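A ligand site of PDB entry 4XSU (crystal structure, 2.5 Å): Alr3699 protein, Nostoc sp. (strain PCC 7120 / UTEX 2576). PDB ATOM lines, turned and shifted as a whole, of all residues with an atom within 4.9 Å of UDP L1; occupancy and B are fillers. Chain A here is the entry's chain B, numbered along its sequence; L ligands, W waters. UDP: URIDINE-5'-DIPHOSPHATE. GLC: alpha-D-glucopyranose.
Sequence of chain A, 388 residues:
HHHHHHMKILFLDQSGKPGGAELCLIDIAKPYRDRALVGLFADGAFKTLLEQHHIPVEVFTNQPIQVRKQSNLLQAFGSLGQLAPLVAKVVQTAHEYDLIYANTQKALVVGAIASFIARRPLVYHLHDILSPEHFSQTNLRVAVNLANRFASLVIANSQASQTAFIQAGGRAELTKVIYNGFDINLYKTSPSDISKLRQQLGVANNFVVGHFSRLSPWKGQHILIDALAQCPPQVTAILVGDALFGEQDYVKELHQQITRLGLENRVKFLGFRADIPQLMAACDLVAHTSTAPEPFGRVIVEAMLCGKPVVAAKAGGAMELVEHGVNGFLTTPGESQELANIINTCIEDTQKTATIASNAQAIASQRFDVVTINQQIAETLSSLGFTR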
ATOM      1  N   PRO A  18     -20.550 -22.076   0.241  1.00  0.00           N
ATOM      2  CA  PRO A  18     -21.283 -23.296   0.615  1.00  0.00           C
ATOM      3  C   PRO A  18     -20.989 -23.741   2.064  1.00  0.00           C
ATOM      4  O   PRO A  18     -20.264 -24.694   2.307  1.00  0.00           O
ATOM      5  CB  PRO A  18     -20.772 -24.308  -0.403  1.00  0.00           C
ATOM      6  CG  PRO A  18     -19.364 -23.887  -0.653  1.00  0.00           C
ATOM      7  CD  PRO A  18     -19.368 -22.381  -0.581  1.00  0.00           C
ATOM      8  N   GLY A  19     -21.558 -23.004   3.017  1.00  0.00           N
ATOM      9  CA  GLY A  19     -21.488 -23.334   4.422  1.00  0.00           C
ATOM     10  C   GLY A  19     -22.494 -24.433   4.724  1.00  0.00           C
ATOM     11  O   GLY A  19     -23.217 -24.948   3.820  1.00  0.00           O
ATOM     12  N   GLY A  20     -22.545 -24.794   5.992  1.00  0.00           N
ATOM     13  CA  GLY A  20     -23.466 -25.831   6.457  1.00  0.00           C
ATOM     14  C   GLY A  20     -24.915 -25.582   6.111  1.00  0.00           C
ATOM     15  O   GLY A  20     -25.606 -26.473   5.601  1.00  0.00           O
ATOM     16  N   ALA A  21     -25.398 -24.364   6.375  1.00  0.00           N
ATOM     17  CA  ALA A  21     -26.811 -24.066   6.142  1.00  0.00           C
ATOM     18  C   ALA A  21     -27.083 -24.176   4.672  1.00  0.00           C
ATOM     19  O   ALA A  21     -28.108 -24.698   4.251  1.00  0.00           O
ATOM     20  CB  ALA A  21     -27.164 -22.692   6.636  1.00  0.00           C
ATOM     21  N   LEU A  23     -25.293 -25.939   2.273  1.00  0.00           N
ATOM     22  CA  LEU A  23     -25.318 -27.361   1.877  1.00  0.00           C
ATOM     23  C   LEU A  23     -26.608 -28.012   2.273  1.00  0.00           C
ATOM     24  O   LEU A  23     -27.211 -28.736   1.477  1.00  0.00           O
ATOM     25  CB  LEU A  23     -24.135 -28.130   2.467  1.00  0.00           C
ATOM     26  CG  LEU A  23     -22.801 -27.658   1.849  1.00  0.00           C
ATOM     27  CD1 LEU A  23     -21.616 -27.956   2.754  1.00  0.00           C
ATOM     28  CD2 LEU A  23     -22.648 -28.263   0.481  1.00  0.00           C
ATOM     29  N   PHE A 212     -13.044 -31.482  10.338  1.00  0.00           N
ATOM     30  CA  PHE A 212     -13.677 -30.995   9.135  1.00  0.00           C
ATOM     31  C   PHE A 212     -14.533 -29.738   9.351  1.00  0.00           C
ATOM     32  O   PHE A 212     -15.718 -29.705   9.048  1.00  0.00           O
ATOM     33  CB  PHE A 212     -14.529 -32.087   8.547  1.00  0.00           C
ATOM     34  CG  PHE A 212     -13.748 -33.246   8.100  1.00  0.00           C
ATOM     35  CD1 PHE A 212     -13.304 -34.195   9.015  1.00  0.00           C
ATOM     36  CD2 PHE A 212     -13.412 -33.393   6.763  1.00  0.00           C
ATOM     37  CE1 PHE A 212     -12.573 -35.274   8.596  1.00  0.00           C
ATOM     38  CE2 PHE A 212     -12.680 -34.473   6.344  1.00  0.00           C
ATOM     39  CZ  PHE A 212     -12.269 -35.421   7.263  1.00  0.00           C
ATOM     40  N   SER A 213     -13.914 -28.667   9.812  1.00  0.00           N
ATOM     41  CA  SER A 213     -14.647 -27.459  10.068  1.00  0.00           C
ATOM     42  C   SER A 213     -13.928 -26.229   9.549  1.00  0.00           C
ATOM     43  O   SER A 213     -12.703 -26.169   9.541  1.00  0.00           O
ATOM     44  CB  SER A 213     -14.790 -27.312  11.543  1.00  0.00           C
ATOM     45  OG  SER A 213     -15.317 -26.055  11.812  1.00  0.00           O
ATOM     46  N   ARG A 214     -14.704 -25.233   9.136  1.00  0.00           N
ATOM     47  CA  ARG A 214     -14.126 -23.954   8.768  1.00  0.00           C
ATOM     48  C   ARG A 214     -13.291 -23.434   9.939  1.00  0.00           C
ATOM     49  O   ARG A 214     -13.540 -23.756  11.091  1.00  0.00           O
ATOM     50  CB  ARG A 214     -15.219 -22.966   8.366  1.00  0.00           C
ATOM     51  CG  ARG A 214     -16.064 -22.460   9.524  1.00  0.00           C
ATOM     52  CD  ARG A 214     -17.374 -21.844   9.040  1.00  0.00           C
ATOM     53  NE  ARG A 214     -17.956 -21.020  10.090  1.00  0.00           N
ATOM     54  CZ  ARG A 214     -19.048 -21.321  10.788  1.00  0.00           C
ATOM     55  NH1 ARG A 214     -19.707 -22.420  10.552  1.00  0.00           N
ATOM     56  NH2 ARG A 214     -19.483 -20.483  11.723  1.00  0.00           N
ATOM     57  N   TRP A 218     -14.215 -20.531  17.333  1.00  0.00           N
ATOM     58  CA  TRP A 218     -15.268 -21.257  18.013  1.00  0.00           C
ATOM     59  C   TRP A 218     -15.406 -22.688  17.513  1.00  0.00           C
ATOM     60  O   TRP A 218     -16.070 -23.500  18.168  1.00  0.00           O
ATOM     61  CB  TRP A 218     -16.615 -20.488  17.995  1.00  0.00           C
ATOM     62  CG  TRP A 218     -17.483 -20.672  16.784  1.00  0.00           C
ATOM     63  CD1 TRP A 218     -17.463 -19.918  15.644  1.00  0.00           C
ATOM     64  CD2 TRP A 218     -18.541 -21.637  16.606  1.00  0.00           C
ATOM     65  NE1 TRP A 218     -18.418 -20.375  14.752  1.00  0.00           N
ATOM     66  CE2 TRP A 218     -19.092 -21.427  15.325  1.00  0.00           C
ATOM     67  CE3 TRP A 218     -19.049 -22.689  17.394  1.00  0.00           C
ATOM     68  CZ2 TRP A 218     -20.136 -22.222  14.806  1.00  0.00           C
ATOM     69  CZ3 TRP A 218     -20.087 -23.472  16.878  1.00  0.00           C
ATOM     70  CH2 TRP A 218     -20.613 -23.234  15.593  1.00  0.00           C
ATOM     71  N   LYS A 219     -14.799 -23.003  16.366  1.00  0.00           N
ATOM     72  CA  LYS A 219     -14.736 -24.388  15.908  1.00  0.00           C
ATOM     73  C   LYS A 219     -13.637 -25.216  16.620  1.00  0.00           C
ATOM     74  O   LYS A 219     -13.585 -26.425  16.480  1.00  0.00           O
ATOM     75  CB  LYS A 219     -14.587 -24.449  14.389  1.00  0.00           C
ATOM     76  CG  LYS A 219     -15.794 -23.921  13.632  1.00  0.00           C
ATOM     77  CD  LYS A 219     -17.050 -24.706  13.942  1.00  0.00           C
ATOM     78  CE  LYS A 219     -18.051 -24.567  12.835  1.00  0.00           C
ATOM     79  NZ  LYS A 219     -19.332 -25.255  13.138  1.00  0.00           N
ATOM     80  N   VAL A 240      -9.383 -29.820   7.778  1.00  0.00           N
ATOM     81  CA  VAL A 240     -10.013 -29.622   6.490  1.00  0.00           C
ATOM     82  C   VAL A 240     -11.039 -28.516   6.662  1.00  0.00           C
ATOM     83  O   VAL A 240     -12.008 -28.658   7.416  1.00  0.00           O
ATOM     84  CB  VAL A 240     -10.684 -30.884   6.025  1.00  0.00           C
ATOM     85  CG1 VAL A 240     -11.239 -30.713   4.617  1.00  0.00           C
ATOM     86  CG2 VAL A 240      -9.682 -32.023   6.060  1.00  0.00           C
ATOM     87  N   GLY A 241     -10.788 -27.404   5.953  1.00  0.00           N
ATOM     88  CA  GLY A 241     -11.625 -26.220   5.983  1.00  0.00           C
ATOM     89  C   GLY A 241     -10.943 -24.919   5.545  1.00  0.00           C
ATOM     90  O   GLY A 241      -9.722 -24.787   5.511  1.00  0.00           O
ATOM     91  N   ASP A 242     -11.794 -23.949   5.269  1.00  0.00           N
ATOM     92  CA  ASP A 242     -11.427 -22.663   4.739  1.00  0.00           C
ATOM     93  C   ASP A 242     -11.372 -21.701   5.900  1.00  0.00           C
ATOM     94  O   ASP A 242     -12.144 -21.855   6.844  1.00  0.00           O
ATOM     95  CB  ASP A 242     -12.547 -22.188   3.790  1.00  0.00           C
ATOM     96  CG  ASP A 242     -12.004 -21.633   2.498  1.00  0.00           C
ATOM     97  OD1 ASP A 242     -10.778 -21.455   2.378  1.00  0.00           O
ATOM     98  OD2 ASP A 242     -12.833 -21.398   1.595  1.00  0.00           O
ATOM     99  N   GLY A 271      -6.954 -27.066   3.378  1.00  0.00           N
ATOM    100  CA  GLY A 271      -7.988 -26.093   2.966  1.00  0.00           C
ATOM    101  C   GLY A 271      -9.328 -26.706   2.601  1.00  0.00           C
ATOM    102  O   GLY A 271      -9.643 -27.867   2.926  1.00  0.00           O
ATOM    103  N   PHE A 272     -10.143 -25.953   1.895  1.00  0.00           N
ATOM    104  CA  PHE A 272     -11.468 -26.408   1.597  1.00  0.00           C
ATOM    105  C   PHE A 272     -11.383 -27.532   0.592  1.00  0.00           C
ATOM    106  O   PHE A 272     -10.652 -27.442  -0.375  1.00  0.00           O
ATOM    107  CB  PHE A 272     -12.342 -25.291   1.043  1.00  0.00           C
ATOM    108  CG  PHE A 272     -13.811 -25.667   0.917  1.00  0.00           C
ATOM    109  CD1 PHE A 272     -14.683 -25.447   1.985  1.00  0.00           C
ATOM    110  CD2 PHE A 272     -14.299 -26.253  -0.254  1.00  0.00           C
ATOM    111  CE1 PHE A 272     -16.018 -25.775   1.869  1.00  0.00           C
ATOM    112  CE2 PHE A 272     -15.644 -26.584  -0.373  1.00  0.00           C
ATOM    113  CZ  PHE A 272     -16.498 -26.338   0.680  1.00  0.00           C
ATOM    114  N   ARG A 273     -12.193 -28.562   0.824  1.00  0.00           N
ATOM    115  CA  ARG A 273     -12.198 -29.748   0.021  1.00  0.00           C
ATOM    116  C   ARG A 273     -13.623 -30.223  -0.226  1.00  0.00           C
ATOM    117  O   ARG A 273     -14.467 -30.115   0.654  1.00  0.00           O
ATOM    118  CB  ARG A 273     -11.465 -30.849   0.774  1.00  0.00           C
ATOM    119  CG  ARG A 273      -9.967 -30.612   0.945  1.00  0.00           C
ATOM    120  CD  ARG A 273      -9.237 -30.918  -0.341  1.00  0.00           C
ATOM    121  NE  ARG A 273      -9.304 -32.344  -0.684  1.00  0.00           N
ATOM    122  CZ  ARG A 273      -8.249 -33.165  -0.674  1.00  0.00           C
ATOM    123  NH1 ARG A 273      -8.421 -34.444  -1.016  1.00  0.00           N
ATOM    124  NH2 ARG A 273      -7.030 -32.731  -0.346  1.00  0.00           N
ATOM    125  N   ALA A 274     -13.863 -30.791  -1.390  1.00  0.00           N
ATOM    126  CA  ALA A 274     -15.179 -31.315  -1.744  1.00  0.00           C
ATOM    127  C   ALA A 274     -15.290 -32.820  -1.520  1.00  0.00           C
ATOM    128  O   ALA A 274     -16.400 -33.348  -1.488  1.00  0.00           O
ATOM    129  CB  ALA A 274     -15.472 -31.015  -3.204  1.00  0.00           C
ATOM    130  N   ILE A 276     -15.269 -34.984   0.941  1.00  0.00           N
ATOM    131  CA  ILE A 276     -15.360 -35.123   2.403  1.00  0.00           C
ATOM    132  C   ILE A 276     -15.601 -36.568   2.852  1.00  0.00           C
ATOM    133  O   ILE A 276     -14.900 -37.077   3.719  1.00  0.00           O
ATOM    134  CB  ILE A 276     -16.428 -34.177   3.034  1.00  0.00           C
ATOM    135  CG1 ILE A 276     -16.089 -32.708   2.738  1.00  0.00           C
ATOM    136  CG2 ILE A 276     -16.507 -34.387   4.533  1.00  0.00           C
ATOM    137  CD1 ILE A 276     -14.713 -32.264   3.209  1.00  0.00           C
ATOM    138  N   GLU A 294     -22.900 -26.167  19.310  1.00  0.00           N
ATOM    139  CA  GLU A 294     -23.142 -26.396  17.908  1.00  0.00           C
ATOM    140  C   GLU A 294     -24.624 -26.532  17.627  1.00  0.00           C
ATOM    141  O   GLU A 294     -25.319 -27.341  18.225  1.00  0.00           O
ATOM    142  CB  GLU A 294     -22.437 -27.690  17.446  1.00  0.00           C
ATOM    143  CG  GLU A 294     -22.454 -27.955  15.930  1.00  0.00           C
ATOM    144  CD  GLU A 294     -21.430 -27.110  15.183  1.00  0.00           C
ATOM    145  OE1 GLU A 294     -20.275 -27.012  15.706  1.00  0.00           O
ATOM    146  OE2 GLU A 294     -21.785 -26.537  14.100  1.00  0.00           O
ATOM    147  N   GLY A 297     -24.189 -29.677  13.500  1.00  0.00           N
ATOM    148  CA  GLY A 297     -22.882 -30.348  13.325  1.00  0.00           C
ATOM    149  C   GLY A 297     -22.969 -31.415  12.252  1.00  0.00           C
ATOM    150  O   GLY A 297     -23.016 -32.592  12.534  1.00  0.00           O
ATOM    151  N   ARG A 298     -23.054 -30.999  11.003  1.00  0.00           N
ATOM    152  CA  ARG A 298     -23.189 -31.925   9.922  1.00  0.00           C
ATOM    153  C   ARG A 298     -22.030 -32.943   9.854  1.00  0.00           C
ATOM    154  O   ARG A 298     -22.200 -34.072   9.403  1.00  0.00           O
ATOM    155  CB  ARG A 298     -23.245 -31.155   8.616  1.00  0.00           C
ATOM    156  CG  ARG A 298     -24.564 -30.506   8.328  1.00  0.00           C
ATOM    157  CD  ARG A 298     -24.425 -29.549   7.156  1.00  0.00           C
ATOM    158  NE  ARG A 298     -24.274 -30.262   5.891  1.00  0.00           N
ATOM    159  CZ  ARG A 298     -25.258 -30.796   5.191  1.00  0.00           C
ATOM    160  NH1 ARG A 298     -26.527 -30.723   5.579  1.00  0.00           N
ATOM    161  NH2 ARG A 298     -24.981 -31.424   4.069  1.00  0.00           N
ATOM    162  N   VAL A 299     -20.834 -32.517  10.248  1.00  0.00           N
ATOM    163  CA  VAL A 299     -19.667 -33.376  10.134  1.00  0.00           C
ATOM    164  C   VAL A 299     -19.755 -34.592  11.059  1.00  0.00           C
ATOM    165  O   VAL A 299     -19.235 -35.662  10.723  1.00  0.00           O
ATOM    166  CB  VAL A 299     -18.368 -32.615  10.401  1.00  0.00           C
ATOM    167  CG1 VAL A 299     -18.100 -31.633   9.286  1.00  0.00           C
ATOM    168  CG2 VAL A 299     -18.380 -31.885  11.735  1.00  0.00           C
ATOM    169  N   GLU A 302     -22.009 -36.927   9.236  1.00  0.00           N
ATOM    170  CA  GLU A 302     -21.294 -37.418   8.065  1.00  0.00           C
ATOM    171  C   GLU A 302     -20.321 -38.524   8.496  1.00  0.00           C
ATOM    172  O   GLU A 302     -20.297 -39.583   7.883  1.00  0.00           O
ATOM    173  CB  GLU A 302     -20.557 -36.261   7.360  1.00  0.00           C
ATOM    174  CG  GLU A 302     -21.487 -35.401   6.509  1.00  0.00           C
ATOM    175  CD  GLU A 302     -20.915 -34.010   6.169  1.00  0.00           C
ATOM    176  OE1 GLU A 302     -21.479 -33.347   5.300  1.00  0.00           O
ATOM    177  OE2 GLU A 302     -19.912 -33.583   6.772  1.00  0.00           O
HETATM  178  N1  UDP L   1     -17.489 -29.097   4.402  1.00  0.00           N
HETATM  179  C2  UDP L   1     -16.773 -29.150   3.196  1.00  0.00           C
HETATM  180  N3  UDP L   1     -15.472 -28.848   3.161  1.00  0.00           N
HETATM  181  C4  UDP L   1     -14.835 -28.488   4.281  1.00  0.00           C
HETATM  182  C5  UDP L   1     -15.509 -28.434   5.485  1.00  0.00           C
HETATM  183  C6  UDP L   1     -16.864 -28.741   5.530  1.00  0.00           C
HETATM  184  O2  UDP L   1     -17.358 -29.476   2.139  1.00  0.00           O
HETATM  185  O4  UDP L   1     -13.611 -28.209   4.239  1.00  0.00           O
HETATM  186  C1' UDP L   1     -18.919 -29.425   4.431  1.00  0.00           C
HETATM  187  C2' UDP L   1     -19.136 -30.695   5.236  1.00  0.00           C
HETATM  188  O2' UDP L   1     -19.763 -31.696   4.422  1.00  0.00           O
HETATM  189  C3' UDP L   1     -20.038 -30.320   6.392  1.00  0.00           C
HETATM  190  C4' UDP L   1     -20.336 -28.840   6.232  1.00  0.00           C
HETATM  191  O4' UDP L   1     -19.647 -28.371   5.064  1.00  0.00           O
HETATM  192  O3' UDP L   1     -21.254 -31.073   6.325  1.00  0.00           O
HETATM  193  C5' UDP L   1     -19.873 -28.054   7.456  1.00  0.00           C
HETATM  194  O5' UDP L   1     -21.003 -27.682   8.243  1.00  0.00           O
HETATM  195  PA  UDP L   1     -20.949 -27.804   9.846  1.00  0.00           P
HETATM  196  O1A UDP L   1     -19.967 -28.895  10.208  1.00  0.00           O
HETATM  197  O2A UDP L   1     -22.374 -27.873  10.357  1.00  0.00           O
HETATM  198  O3A UDP L   1     -20.327 -26.388  10.284  1.00  0.00           O
HETATM  199  PB  UDP L   1     -21.082 -25.014   9.927  1.00  0.00           P
HETATM  200  O1B UDP L   1     -20.133 -24.320   8.979  1.00  0.00           O
HETATM  201  O2B UDP L   1     -22.383 -25.463   9.306  1.00  0.00           O
HETATM  202  O3B UDP L   1     -21.243 -24.326  11.270  1.00  0.00           O
HETATM  203  C1  GLC L   2     -25.517 -23.952  10.981  1.00  0.00           C
HETATM  204  C2  GLC L   2     -24.673 -24.501  12.127  1.00  0.00           C
HETATM  205  C3  GLC L   2     -24.345 -25.986  11.996  1.00  0.00           C
HETATM  206  C4  GLC L   2     -25.483 -26.688  11.294  1.00  0.00           C
HETATM  207  C5  GLC L   2     -25.576 -26.198   9.887  1.00  0.00           C
HETATM  208  C6  GLC L   2     -26.683 -26.984   9.154  1.00  0.00           C
HETATM  209  O1  GLC L   2     -24.819 -22.891  10.332  1.00  0.00           O
HETATM  210  O2  GLC L   2     -23.554 -23.647  12.419  1.00  0.00           O
HETATM  211  O3  GLC L   2     -24.162 -26.624  13.275  1.00  0.00           O
HETATM  212  O4  GLC L   2     -25.178 -28.053  11.118  1.00  0.00           O
HETATM  213  O5  GLC L   2     -26.078 -24.920  10.060  1.00  0.00           O
HETATM  214  O6  GLC L   2     -27.941 -26.844   9.846  1.00  0.00           O
HETATM  215  O   HOH W   1     -18.565 -25.514   4.430  1.00  0.00           O
HETATM  216  O   HOH W   2     -22.333 -32.486   2.942  1.00  0.00           O
HETATM  217  O   HOH W   3     -19.055 -31.015  -0.462  1.00  0.00           O
HETATM  218  O   HOH W   4     -23.876 -23.024   7.967  1.00  0.00           O
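The side-chain carboxylate (OE2) of Glu 294 lies within salt-bridge range of the side-chain amino group (NZ) of Lys 219 (2.9 Å).
The backbone NH (N) of Gly 241 is in hydrogen-bond range of the backbone carbonyl oxygen (O) of Gly 271.
The backbone carbonyl oxygen (O) of Val 240 lies within hydrogen-bond range of the backbone NH (N) of Ser 213 (3.1 Å).
Water W2 lies within hydrogen-bond range of the side-chain carboxylate (OE1) of Glu 302, the guanidinium group (NH2) of Arg 298 and an oxygen (O2') of UDP L1.
Water W1 lies within hydrogen-bond range of O of Pro 18 (2.8 Å) and O4' of UDP L1 (3.1 Å).
Water W4 lies within hydrogen-bond range of an oxygen (O1) of GLC L2 (2.5 Å), the backbone NH of Ala 21 (2.6 Å), the backbone NH of Gly 20 (3.0 Å) and an oxygen (O2B) of UDP L1 (3.2 Å).
Leu 23 touches UDP L1.
Phe 212 touches UDP L1.
CG1 of Val 240 touches O4 of UDP L1, 3.5 Å away.
CE1 of Phe 272 touches N3 of UDP L1 (3.4 Å).
Ile 276 touches UDP L1 (CD1 to N3, 3.5 Å).
Glu 294 touches UDP L1.
Gly 297 touches UDP L1.
Val 299 touches UDP L1.
Hydrophobic or aromatic side chains within 4 Å of UDP L1: Leu 23, Val 240, Phe 272, Ile 276 and Val 299.
15 residues have an atom within 4 Å of UDP L1: Gly 20, Leu 23, Phe 212, Arg 214, Lys 219, Val 240, Gly 241, Phe 272, Arg 273, Ile 276, Glu 294, Gly 297, Arg 298, Val 299 and Glu 302.
Along chain A the residues within 4 Å of UDP L1 span positions 20 to 302.
The nearest printed residue that does not touch UDP L1 is Gly 271 (4.2 Å).
The guanidinium group of Arg 214 lies within salt-bridge range of an oxygen (O1B) of UDP L1 (2.5 Å).
An oxygen (O3') of UDP L1 is in hydrogen-bond range of the side-chain carboxylate (OE1) of Glu 302 (2.5 Å).
The side-chain amino group (NZ) of Lys 219 is in salt-bridge range of an oxygen (O3B) of UDP L1 (2.8 Å).
The backbone carbonyl oxygen of Arg 273 is in hydrogen-bond range of a nitrogen (N3) of UDP L1 (3.0 Å).
O2A of UDP L1 lies within hydrogen-bond range of N of Arg 298 (3.3 Å).
An oxygen (O3') of UDP L1 lies close to the guanidinium group of Arg 298 (3.2 Å).
O2B of UDP L1 sits close to N of Gly 20 (3.4 Å).
The backbone NH of Gly 241 sits close to an oxygen (O4) of UDP L1 (3.4 Å).
The side-chain carboxylate (OE2) of Glu 294 lies within hydrogen-bond range of an oxygen (O3) of GLC L2 (2.5 Å).
The backbone NH (N) of Gly 297 is in hydrogen-bond range of an oxygen (O4) of GLC L2 (3.0 Å).
An oxygen (O3B) of UDP L1 sits at hydrogen-bond distance from an oxygen (O2) of GLC L2 (2.7 Å).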
